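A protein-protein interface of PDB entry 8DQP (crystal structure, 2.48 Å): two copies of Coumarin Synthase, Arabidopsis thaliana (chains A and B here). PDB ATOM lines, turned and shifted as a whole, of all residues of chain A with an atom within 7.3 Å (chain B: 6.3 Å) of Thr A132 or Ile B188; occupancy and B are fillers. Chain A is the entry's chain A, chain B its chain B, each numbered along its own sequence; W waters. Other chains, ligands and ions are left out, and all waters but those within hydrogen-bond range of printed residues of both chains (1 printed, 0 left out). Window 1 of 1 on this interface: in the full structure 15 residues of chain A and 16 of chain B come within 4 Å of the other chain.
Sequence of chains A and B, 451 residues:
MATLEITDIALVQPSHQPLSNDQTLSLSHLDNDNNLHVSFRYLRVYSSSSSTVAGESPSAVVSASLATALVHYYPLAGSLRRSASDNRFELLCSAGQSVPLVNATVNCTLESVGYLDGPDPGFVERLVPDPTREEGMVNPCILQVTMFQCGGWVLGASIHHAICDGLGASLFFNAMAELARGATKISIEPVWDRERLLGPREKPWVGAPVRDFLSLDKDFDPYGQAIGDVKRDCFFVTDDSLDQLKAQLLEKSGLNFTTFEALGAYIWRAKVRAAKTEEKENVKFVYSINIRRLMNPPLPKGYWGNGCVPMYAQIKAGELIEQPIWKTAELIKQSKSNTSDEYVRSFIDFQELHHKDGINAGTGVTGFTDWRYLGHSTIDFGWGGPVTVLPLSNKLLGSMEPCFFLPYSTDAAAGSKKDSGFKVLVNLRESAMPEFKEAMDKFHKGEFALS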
ATOM      1  N   HIS A  37      24.655   8.542  -5.897  1.00  0.00           N
ATOM      2  CA  HIS A  37      24.385   9.178  -4.573  1.00  0.00           C
ATOM      3  C   HIS A  37      22.908   9.572  -4.524  1.00  0.00           C
ATOM      4  O   HIS A  37      22.586  10.719  -4.752  1.00  0.00           O
ATOM      5  CB  HIS A  37      25.188  10.462  -4.382  1.00  0.00           C
ATOM      6  CG  HIS A  37      24.989  11.086  -3.053  1.00  0.00           C
ATOM      7  ND1 HIS A  37      24.524  10.333  -1.935  1.00  0.00           N
ATOM      8  CD2 HIS A  37      25.244  12.364  -2.614  1.00  0.00           C
ATOM      9  CE1 HIS A  37      24.528  11.126  -0.863  1.00  0.00           C
ATOM     10  NE2 HIS A  37      24.961  12.414  -1.250  1.00  0.00           N
ATOM     11  N   VAL A  38      22.075   8.540  -4.409  1.00  0.00           N
ATOM     12  CA  VAL A  38      20.661   8.542  -4.453  1.00  0.00           C
ATOM     13  C   VAL A  38      20.145   7.275  -3.767  1.00  0.00           C
ATOM     14  O   VAL A  38      20.844   6.298  -3.667  1.00  0.00           O
ATOM     15  CB  VAL A  38      20.076   8.576  -5.868  1.00  0.00           C
ATOM     16  CG1 VAL A  38      20.303   9.891  -6.547  1.00  0.00           C
ATOM     17  CG2 VAL A  38      20.561   7.443  -6.743  1.00  0.00           C
ATOM     18  N   SER A  39      18.867   7.303  -3.390  1.00  0.00           N
ATOM     19  CA  SER A  39      18.233   6.138  -2.875  1.00  0.00           C
ATOM     20  C   SER A  39      17.512   5.451  -4.002  1.00  0.00           C
ATOM     21  O   SER A  39      16.836   6.081  -4.761  1.00  0.00           O
ATOM     22  CB  SER A  39      17.294   6.500  -1.746  1.00  0.00           C
ATOM     23  OG  SER A  39      18.091   6.818  -0.573  1.00  0.00           O
ATOM     24  N   PRO A 129       9.763   4.290   2.347  1.00  0.00           N
ATOM     25  CA  PRO A 129      10.217   5.603   2.835  1.00  0.00           C
ATOM     26  C   PRO A 129      10.986   6.398   1.763  1.00  0.00           C
ATOM     27  O   PRO A 129      11.502   5.808   0.833  1.00  0.00           O
ATOM     28  CB  PRO A 129      11.032   5.256   4.101  1.00  0.00           C
ATOM     29  CG  PRO A 129      10.443   3.892   4.498  1.00  0.00           C
ATOM     30  CD  PRO A 129      10.346   3.184   3.140  1.00  0.00           C
ATOM     31  N   ASP A 130      11.030   7.731   1.878  1.00  0.00           N
ATOM     32  CA  ASP A 130      11.485   8.584   0.825  1.00  0.00           C
ATOM     33  C   ASP A 130      12.600   9.464   1.337  1.00  0.00           C
ATOM     34  O   ASP A 130      12.511  10.661   1.140  1.00  0.00           O
ATOM     35  CB  ASP A 130      10.368   9.458   0.241  1.00  0.00           C
ATOM     36  CG  ASP A 130      10.722   9.989  -1.147  1.00  0.00           C
ATOM     37  OD1 ASP A 130      11.458   9.262  -1.829  1.00  0.00           O
ATOM     38  OD2 ASP A 130      10.331  11.152  -1.518  1.00  0.00           O
ATOM     39  N   PRO A 131      13.734   8.883   1.800  1.00  0.00           N
ATOM     40  CA  PRO A 131      14.838   9.671   2.345  1.00  0.00           C
ATOM     41  C   PRO A 131      15.400  10.549   1.229  1.00  0.00           C
ATOM     42  O   PRO A 131      15.360  10.108   0.070  1.00  0.00           O
ATOM     43  CB  PRO A 131      15.885   8.616   2.779  1.00  0.00           C
ATOM     44  CG  PRO A 131      15.620   7.420   1.914  1.00  0.00           C
ATOM     45  CD  PRO A 131      14.131   7.471   1.621  1.00  0.00           C
ATOM     46  N   THR A 132      15.888  11.753   1.557  1.00  0.00           N
ATOM     47  CA  THR A 132      16.709  12.570   0.588  1.00  0.00           C
ATOM     48  C   THR A 132      18.106  11.936   0.478  1.00  0.00           C
ATOM     49  O   THR A 132      18.485  11.207   1.480  1.00  0.00           O
ATOM     50  CB  THR A 132      17.022  14.014   1.020  1.00  0.00           C
ATOM     51  OG1 THR A 132      17.838  13.928   2.197  1.00  0.00           O
ATOM     52  CG2 THR A 132      15.818  14.921   1.178  1.00  0.00           C
ATOM     53  N   ARG A 133      18.883  12.247  -0.606  1.00  0.00           N
ATOM     54  CA  ARG A 133      20.228  11.525  -0.816  1.00  0.00           C
ATOM     55  C   ARG A 133      21.026  11.607   0.477  1.00  0.00           C
ATOM     56  O   ARG A 133      21.547  10.560   0.895  1.00  0.00           O
ATOM     57  CB  ARG A 133      21.103  11.982  -1.996  1.00  0.00           C
ATOM     58  CG  ARG A 133      21.516  13.468  -2.060  1.00  0.00           C
ATOM     59  CD  ARG A 133      22.380  13.947  -3.302  1.00  0.00           C
ATOM     60  NE  ARG A 133      21.900  14.702  -4.483  1.00  0.00           N
ATOM     61  CZ  ARG A 133      21.507  16.036  -4.530  1.00  0.00           C
ATOM     62  NH1 ARG A 133      21.570  16.852  -3.449  1.00  0.00           N
ATOM     63  NH2 ARG A 133      20.958  16.521  -5.664  1.00  0.00           N
ATOM     64  N   GLU A 134      21.064  12.808   1.096  1.00  0.00           N
ATOM     65  CA  GLU A 134      21.922  13.007   2.289  1.00  0.00           C
ATOM     66  C   GLU A 134      21.374  12.208   3.479  1.00  0.00           C
ATOM     67  O   GLU A 134      22.107  11.403   4.036  1.00  0.00           O
ATOM     68  CB  GLU A 134      22.104  14.480   2.598  1.00  0.00           C
ATOM     69  CG  GLU A 134      22.875  15.234   1.495  1.00  0.00           C
ATOM     70  CD  GLU A 134      24.359  14.894   1.162  1.00  0.00           C
ATOM     71  OE1 GLU A 134      25.147  14.446   2.145  1.00  0.00           O
ATOM     72  OE2 GLU A 134      24.752  15.074  -0.120  1.00  0.00           O
ATOM     73  N   GLU A 135      20.093  12.388   3.818  1.00  0.00           N
ATOM     74  CA  GLU A 135      19.382  11.563   4.868  1.00  0.00           C
ATOM     75  C   GLU A 135      19.538  10.030   4.659  1.00  0.00           C
ATOM     76  O   GLU A 135      19.503   9.215   5.688  1.00  0.00           O
ATOM     77  CB  GLU A 135      17.878  11.861   4.808  1.00  0.00           C
ATOM     78  CG  GLU A 135      17.425  13.210   5.362  1.00  0.00           C
ATOM     79  CD  GLU A 135      16.167  13.768   4.684  1.00  0.00           C
ATOM     80  OE1 GLU A 135      15.355  12.957   4.059  1.00  0.00           O
ATOM     81  OE2 GLU A 135      16.032  15.040   4.686  1.00  0.00           O
ATOM     82  N   GLY A 136      19.642   9.611   3.367  1.00  0.00           N
ATOM     83  CA  GLY A 136      19.811   8.193   2.976  1.00  0.00           C
ATOM     84  C   GLY A 136      21.148   7.575   3.384  1.00  0.00           C
ATOM     85  O   GLY A 136      21.300   6.364   3.419  1.00  0.00           O
ATOM     86  N   MET A 137      22.120   8.420   3.717  1.00  0.00           N
ATOM     87  CA  MET A 137      23.402   7.982   4.210  1.00  0.00           C
ATOM     88  C   MET A 137      23.300   7.482   5.657  1.00  0.00           C
ATOM     89  O   MET A 137      24.039   6.607   6.101  1.00  0.00           O
ATOM     90  CB  MET A 137      24.416   9.130   4.100  1.00  0.00           C
ATOM     91  CG  MET A 137      24.644   9.591   2.648  1.00  0.00           C
ATOM     92  SD  MET A 137      25.738  11.061   2.456  1.00  0.00           S
ATOM     93  CE  MET A 137      27.147  10.318   3.267  1.00  0.00           C
ATOM     94  N   VAL A 138      22.361   8.042   6.419  1.00  0.00           N
ATOM     95  CA  VAL A 138      22.199   7.698   7.868  1.00  0.00           C
ATOM     96  C   VAL A 138      21.559   6.313   7.975  1.00  0.00           C
ATOM     97  O   VAL A 138      22.028   5.456   8.714  1.00  0.00           O
ATOM     98  CB  VAL A 138      21.374   8.784   8.573  1.00  0.00           C
ATOM     99  CG1 VAL A 138      21.242   8.521  10.052  1.00  0.00           C
ATOM    100  CG2 VAL A 138      21.973  10.162   8.317  1.00  0.00           C
ATOM    101  N   HIS A 160      20.353   2.949  -0.510  1.00  0.00           N
ATOM    102  CA  HIS A 160      21.414   3.838  -1.091  1.00  0.00           C
ATOM    103  C   HIS A 160      22.232   3.076  -2.159  1.00  0.00           C
ATOM    104  O   HIS A 160      22.727   1.986  -1.966  1.00  0.00           O
ATOM    105  CB  HIS A 160      22.343   4.412  -0.004  1.00  0.00           C
ATOM    106  CG  HIS A 160      23.042   5.615  -0.486  1.00  0.00           C
ATOM    107  ND1 HIS A 160      24.109   5.559  -1.290  1.00  0.00           N
ATOM    108  CD2 HIS A 160      22.825   6.928  -0.334  1.00  0.00           C
ATOM    109  CE1 HIS A 160      24.547   6.787  -1.568  1.00  0.00           C
ATOM    110  NE2 HIS A 160      23.774   7.634  -1.058  1.00  0.00           N
ATOM    111  N   TYR B  73      18.538  30.102   5.612  1.00  0.00           N
ATOM    112  CA  TYR B  73      17.464  30.205   6.660  1.00  0.00           C
ATOM    113  C   TYR B  73      17.606  31.501   7.506  1.00  0.00           C
ATOM    114  O   TYR B  73      17.277  31.525   8.699  1.00  0.00           O
ATOM    115  CB  TYR B  73      17.483  28.945   7.528  1.00  0.00           C
ATOM    116  CG  TYR B  73      16.950  27.710   6.858  1.00  0.00           C
ATOM    117  CD1 TYR B  73      15.595  27.523   6.791  1.00  0.00           C
ATOM    118  CD2 TYR B  73      17.754  26.725   6.320  1.00  0.00           C
ATOM    119  CE1 TYR B  73      15.029  26.398   6.228  1.00  0.00           C
ATOM    120  CE2 TYR B  73      17.207  25.579   5.753  1.00  0.00           C
ATOM    121  CZ  TYR B  73      15.831  25.429   5.701  1.00  0.00           C
ATOM    122  OH  TYR B  73      15.115  24.400   5.195  1.00  0.00           O
ATOM    123  N   LEU B 171      12.994  20.663   8.370  1.00  0.00           N
ATOM    124  CA  LEU B 171      13.757  21.062   7.103  1.00  0.00           C
ATOM    125  C   LEU B 171      15.025  21.794   7.516  1.00  0.00           C
ATOM    126  O   LEU B 171      16.062  21.540   6.956  1.00  0.00           O
ATOM    127  CB  LEU B 171      12.978  21.933   6.093  1.00  0.00           C
ATOM    128  CG  LEU B 171      11.982  21.167   5.196  1.00  0.00           C
ATOM    129  CD1 LEU B 171      10.782  22.008   4.736  1.00  0.00           C
ATOM    130  CD2 LEU B 171      12.639  20.527   3.993  1.00  0.00           C
ATOM    131  N   ALA B 175      19.026  20.049   7.315  1.00  0.00           N
ATOM    132  CA  ALA B 175      19.874  20.901   6.531  1.00  0.00           C
ATOM    133  C   ALA B 175      21.182  21.224   7.294  1.00  0.00           C
ATOM    134  O   ALA B 175      22.324  21.127   6.691  1.00  0.00           O
ATOM    135  CB  ALA B 175      19.138  22.147   6.114  1.00  0.00           C
ATOM    136  N   GLU B 178      22.888  17.662   7.670  1.00  0.00           N
ATOM    137  CA  GLU B 178      23.465  17.187   6.426  1.00  0.00           C
ATOM    138  C   GLU B 178      24.777  17.954   6.149  1.00  0.00           C
ATOM    139  O   GLU B 178      25.753  17.283   5.716  1.00  0.00           O
ATOM    140  CB  GLU B 178      22.435  17.152   5.275  1.00  0.00           C
ATOM    141  CG  GLU B 178      22.016  18.511   4.761  1.00  0.00           C
ATOM    142  CD  GLU B 178      21.021  18.513   3.609  1.00  0.00           C
ATOM    143  OE1 GLU B 178      20.652  17.409   3.079  1.00  0.00           O
ATOM    144  OE2 GLU B 178      20.570  19.639   3.287  1.00  0.00           O
ATOM    145  N   LYS B 185      25.973  21.062  -0.407  1.00  0.00           N
ATOM    146  CA  LYS B 185      25.001  22.183  -0.386  1.00  0.00           C
ATOM    147  C   LYS B 185      23.758  21.617   0.330  1.00  0.00           C
ATOM    148  O   LYS B 185      23.660  20.371   0.588  1.00  0.00           O
ATOM    149  CB  LYS B 185      24.711  22.671  -1.822  1.00  0.00           C
ATOM    150  CG  LYS B 185      24.376  21.557  -2.824  1.00  0.00           C
ATOM    151  CD  LYS B 185      23.011  21.703  -3.510  1.00  0.00           C
ATOM    152  CE  LYS B 185      22.560  20.516  -4.361  1.00  0.00           C
ATOM    153  NZ  LYS B 185      22.412  20.845  -5.811  1.00  0.00           N
ATOM    154  N   ILE B 186      22.791  22.480   0.656  1.00  0.00           N
ATOM    155  CA  ILE B 186      21.628  21.954   1.233  1.00  0.00           C
ATOM    156  C   ILE B 186      20.809  21.323   0.092  1.00  0.00           C
ATOM    157  O   ILE B 186      20.832  21.782  -1.028  1.00  0.00           O
ATOM    158  CB  ILE B 186      20.891  23.026   2.058  1.00  0.00           C
ATOM    159  CG1 ILE B 186      20.321  24.122   1.156  1.00  0.00           C
ATOM    160  CG2 ILE B 186      21.791  23.582   3.171  1.00  0.00           C
ATOM    161  CD1 ILE B 186      19.110  24.766   1.715  1.00  0.00           C
ATOM    162  N   SER B 187      20.155  20.205   0.404  1.00  0.00           N
ATOM    163  CA  SER B 187      19.619  19.294  -0.621  1.00  0.00           C
ATOM    164  C   SER B 187      18.178  19.680  -1.043  1.00  0.00           C
ATOM    165  O   SER B 187      17.728  19.479  -2.206  1.00  0.00           O
ATOM    166  CB  SER B 187      19.788  17.845  -0.164  1.00  0.00           C
ATOM    167  OG  SER B 187      18.579  17.219   0.155  1.00  0.00           O
ATOM    168  N   ILE B 188      17.450  20.286  -0.099  1.00  0.00           N
ATOM    169  CA  ILE B 188      16.200  21.005  -0.395  1.00  0.00           C
ATOM    170  C   ILE B 188      16.398  22.486  -0.054  1.00  0.00           C
ATOM    171  O   ILE B 188      16.728  22.803   1.101  1.00  0.00           O
ATOM    172  CB  ILE B 188      15.022  20.406   0.377  1.00  0.00           C
ATOM    173  CG1 ILE B 188      14.859  18.899   0.148  1.00  0.00           C
ATOM    174  CG2 ILE B 188      13.778  21.146  -0.020  1.00  0.00           C
ATOM    175  CD1 ILE B 188      14.277  18.146   1.343  1.00  0.00           C
ATOM    176  N   GLU B 189      16.218  23.361  -1.059  1.00  0.00           N
ATOM    177  CA  GLU B 189      16.461  24.798  -0.921  1.00  0.00           C
ATOM    178  C   GLU B 189      15.156  25.374  -0.396  1.00  0.00           C
ATOM    179  O   GLU B 189      14.124  25.088  -1.000  1.00  0.00           O
ATOM    180  CB  GLU B 189      16.934  25.435  -2.248  1.00  0.00           C
ATOM    181  CG  GLU B 189      17.605  26.811  -2.083  1.00  0.00           C
ATOM    182  CD  GLU B 189      18.616  27.228  -3.188  1.00  0.00           C
ATOM    183  OE1 GLU B 189      19.827  26.781  -3.132  1.00  0.00           O
ATOM    184  OE2 GLU B 189      18.226  28.032  -4.116  1.00  0.00           O
ATOM    185  N   PRO B 190      15.162  26.114   0.760  1.00  0.00           N
ATOM    186  CA  PRO B 190      13.932  26.643   1.358  1.00  0.00           C
ATOM    187  C   PRO B 190      13.233  27.715   0.527  1.00  0.00           C
ATOM    188  O   PRO B 190      13.927  28.651   0.018  1.00  0.00           O
ATOM    189  CB  PRO B 190      14.365  27.326   2.680  1.00  0.00           C
ATOM    190  CG  PRO B 190      15.859  27.587   2.463  1.00  0.00           C
ATOM    191  CD  PRO B 190      16.330  26.430   1.609  1.00  0.00           C
ATOM    192  N   LYS B 301       8.039  21.607  -1.846  1.00  0.00           N
ATOM    193  CA  LYS B 301       8.895  20.691  -1.077  1.00  0.00           C
ATOM    194  C   LYS B 301       9.769  21.508  -0.102  1.00  0.00           C
ATOM    195  O   LYS B 301      10.177  21.011   0.997  1.00  0.00           O
ATOM    196  CB  LYS B 301       9.734  19.882  -2.082  1.00  0.00           C
ATOM    197  CG  LYS B 301      10.787  18.954  -1.479  1.00  0.00           C
ATOM    198  CD  LYS B 301      10.318  17.476  -1.265  1.00  0.00           C
ATOM    199  CE  LYS B 301      10.717  16.832   0.073  1.00  0.00           C
ATOM    200  NZ  LYS B 301       9.756  17.109   1.194  1.00  0.00           N
ATOM    201  N   GLY B 302      10.117  22.742  -0.506  1.00  0.00           N
ATOM    202  CA  GLY B 302      11.030  23.556   0.264  1.00  0.00           C
ATOM    203  C   GLY B 302      10.312  24.412   1.260  1.00  0.00           C
ATOM    204  O   GLY B 302      11.015  25.216   1.915  1.00  0.00           O
ATOM    205  N   TYR B 303       8.961  24.284   1.329  1.00  0.00           N
ATOM    206  CA  TYR B 303       8.142  25.231   2.100  1.00  0.00           C
ATOM    207  C   TYR B 303       8.318  24.942   3.585  1.00  0.00           C
ATOM    208  O   TYR B 303       7.946  23.849   4.012  1.00  0.00           O
ATOM    209  CB  TYR B 303       6.647  25.169   1.761  1.00  0.00           C
ATOM    210  CG  TYR B 303       5.853  26.332   2.345  1.00  0.00           C
ATOM    211  CD1 TYR B 303       5.917  27.612   1.775  1.00  0.00           C
ATOM    212  CD2 TYR B 303       5.091  26.194   3.511  1.00  0.00           C
ATOM    213  CE1 TYR B 303       5.218  28.698   2.304  1.00  0.00           C
ATOM    214  CE2 TYR B 303       4.401  27.272   4.047  1.00  0.00           C
ATOM    215  CZ  TYR B 303       4.444  28.525   3.444  1.00  0.00           C
ATOM    216  OH  TYR B 303       3.762  29.594   3.965  1.00  0.00           O
HETATM  217  O   HOH W   1      18.672  16.097   4.127  1.00  0.00           O
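OE2 of Glu A134 sits at hydrogen-bond distance from NE2 of His A37 (2.9 Å). N of Thr A132 is in hydrogen-bond range of OE1 of Glu A135 (2.8 Å). OE2 of Glu B178 lies within hydrogen-bond range of N of Ser B187.
Thr A132 touches Ser B187 (CB to OG, 3.7 Å). CD1 of Ile B188 touches CG2 of Thr A132, 3.6 Å away. Arg A133 touches Lys B185 (NH1 to CE, 3.9 Å). Ser B187 touches Arg A133 (CB to NH1, 3.9 Å). Glu B178 touches Glu A134 (OE1 to CB, 3.3 Å).
Thr A132 touches two residues of chain B. Of the printed residues of chain A, Ile B188 touches Thr A132 (3.6 Å). Of the printed residues of chain B, Arg A133 touches Lys B185 and Ser B187. Printed residues of chain A within 4 Å of Glu B178: Glu A134. Leu B171 touches none of the printed residues of chain A. Asp A130 touches none of the printed residues of chain B.
Of the 14 printed residues of chain A, 3 touch a printed residue of chain B. Printed residues of chain A that touch a printed residue of chain B: Thr A132, Arg A133 and Glu A134. Along chain A the printed residues that touch a printed residue of chain B span positions 132 to 134. Among the printed residues, 5 pairs touch across the chains.
No position is printed for both chains. Of the 5 pairs that touch across the chains among the printed residues, none has its exchanged pair printed and touching as well.
Water W1 lies within hydrogen-bond range of OE1 of Glu B178 (2.6 Å), OE2 of Glu A135 (2.9 Å) and OG1 of Thr A132 (3.0 Å).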
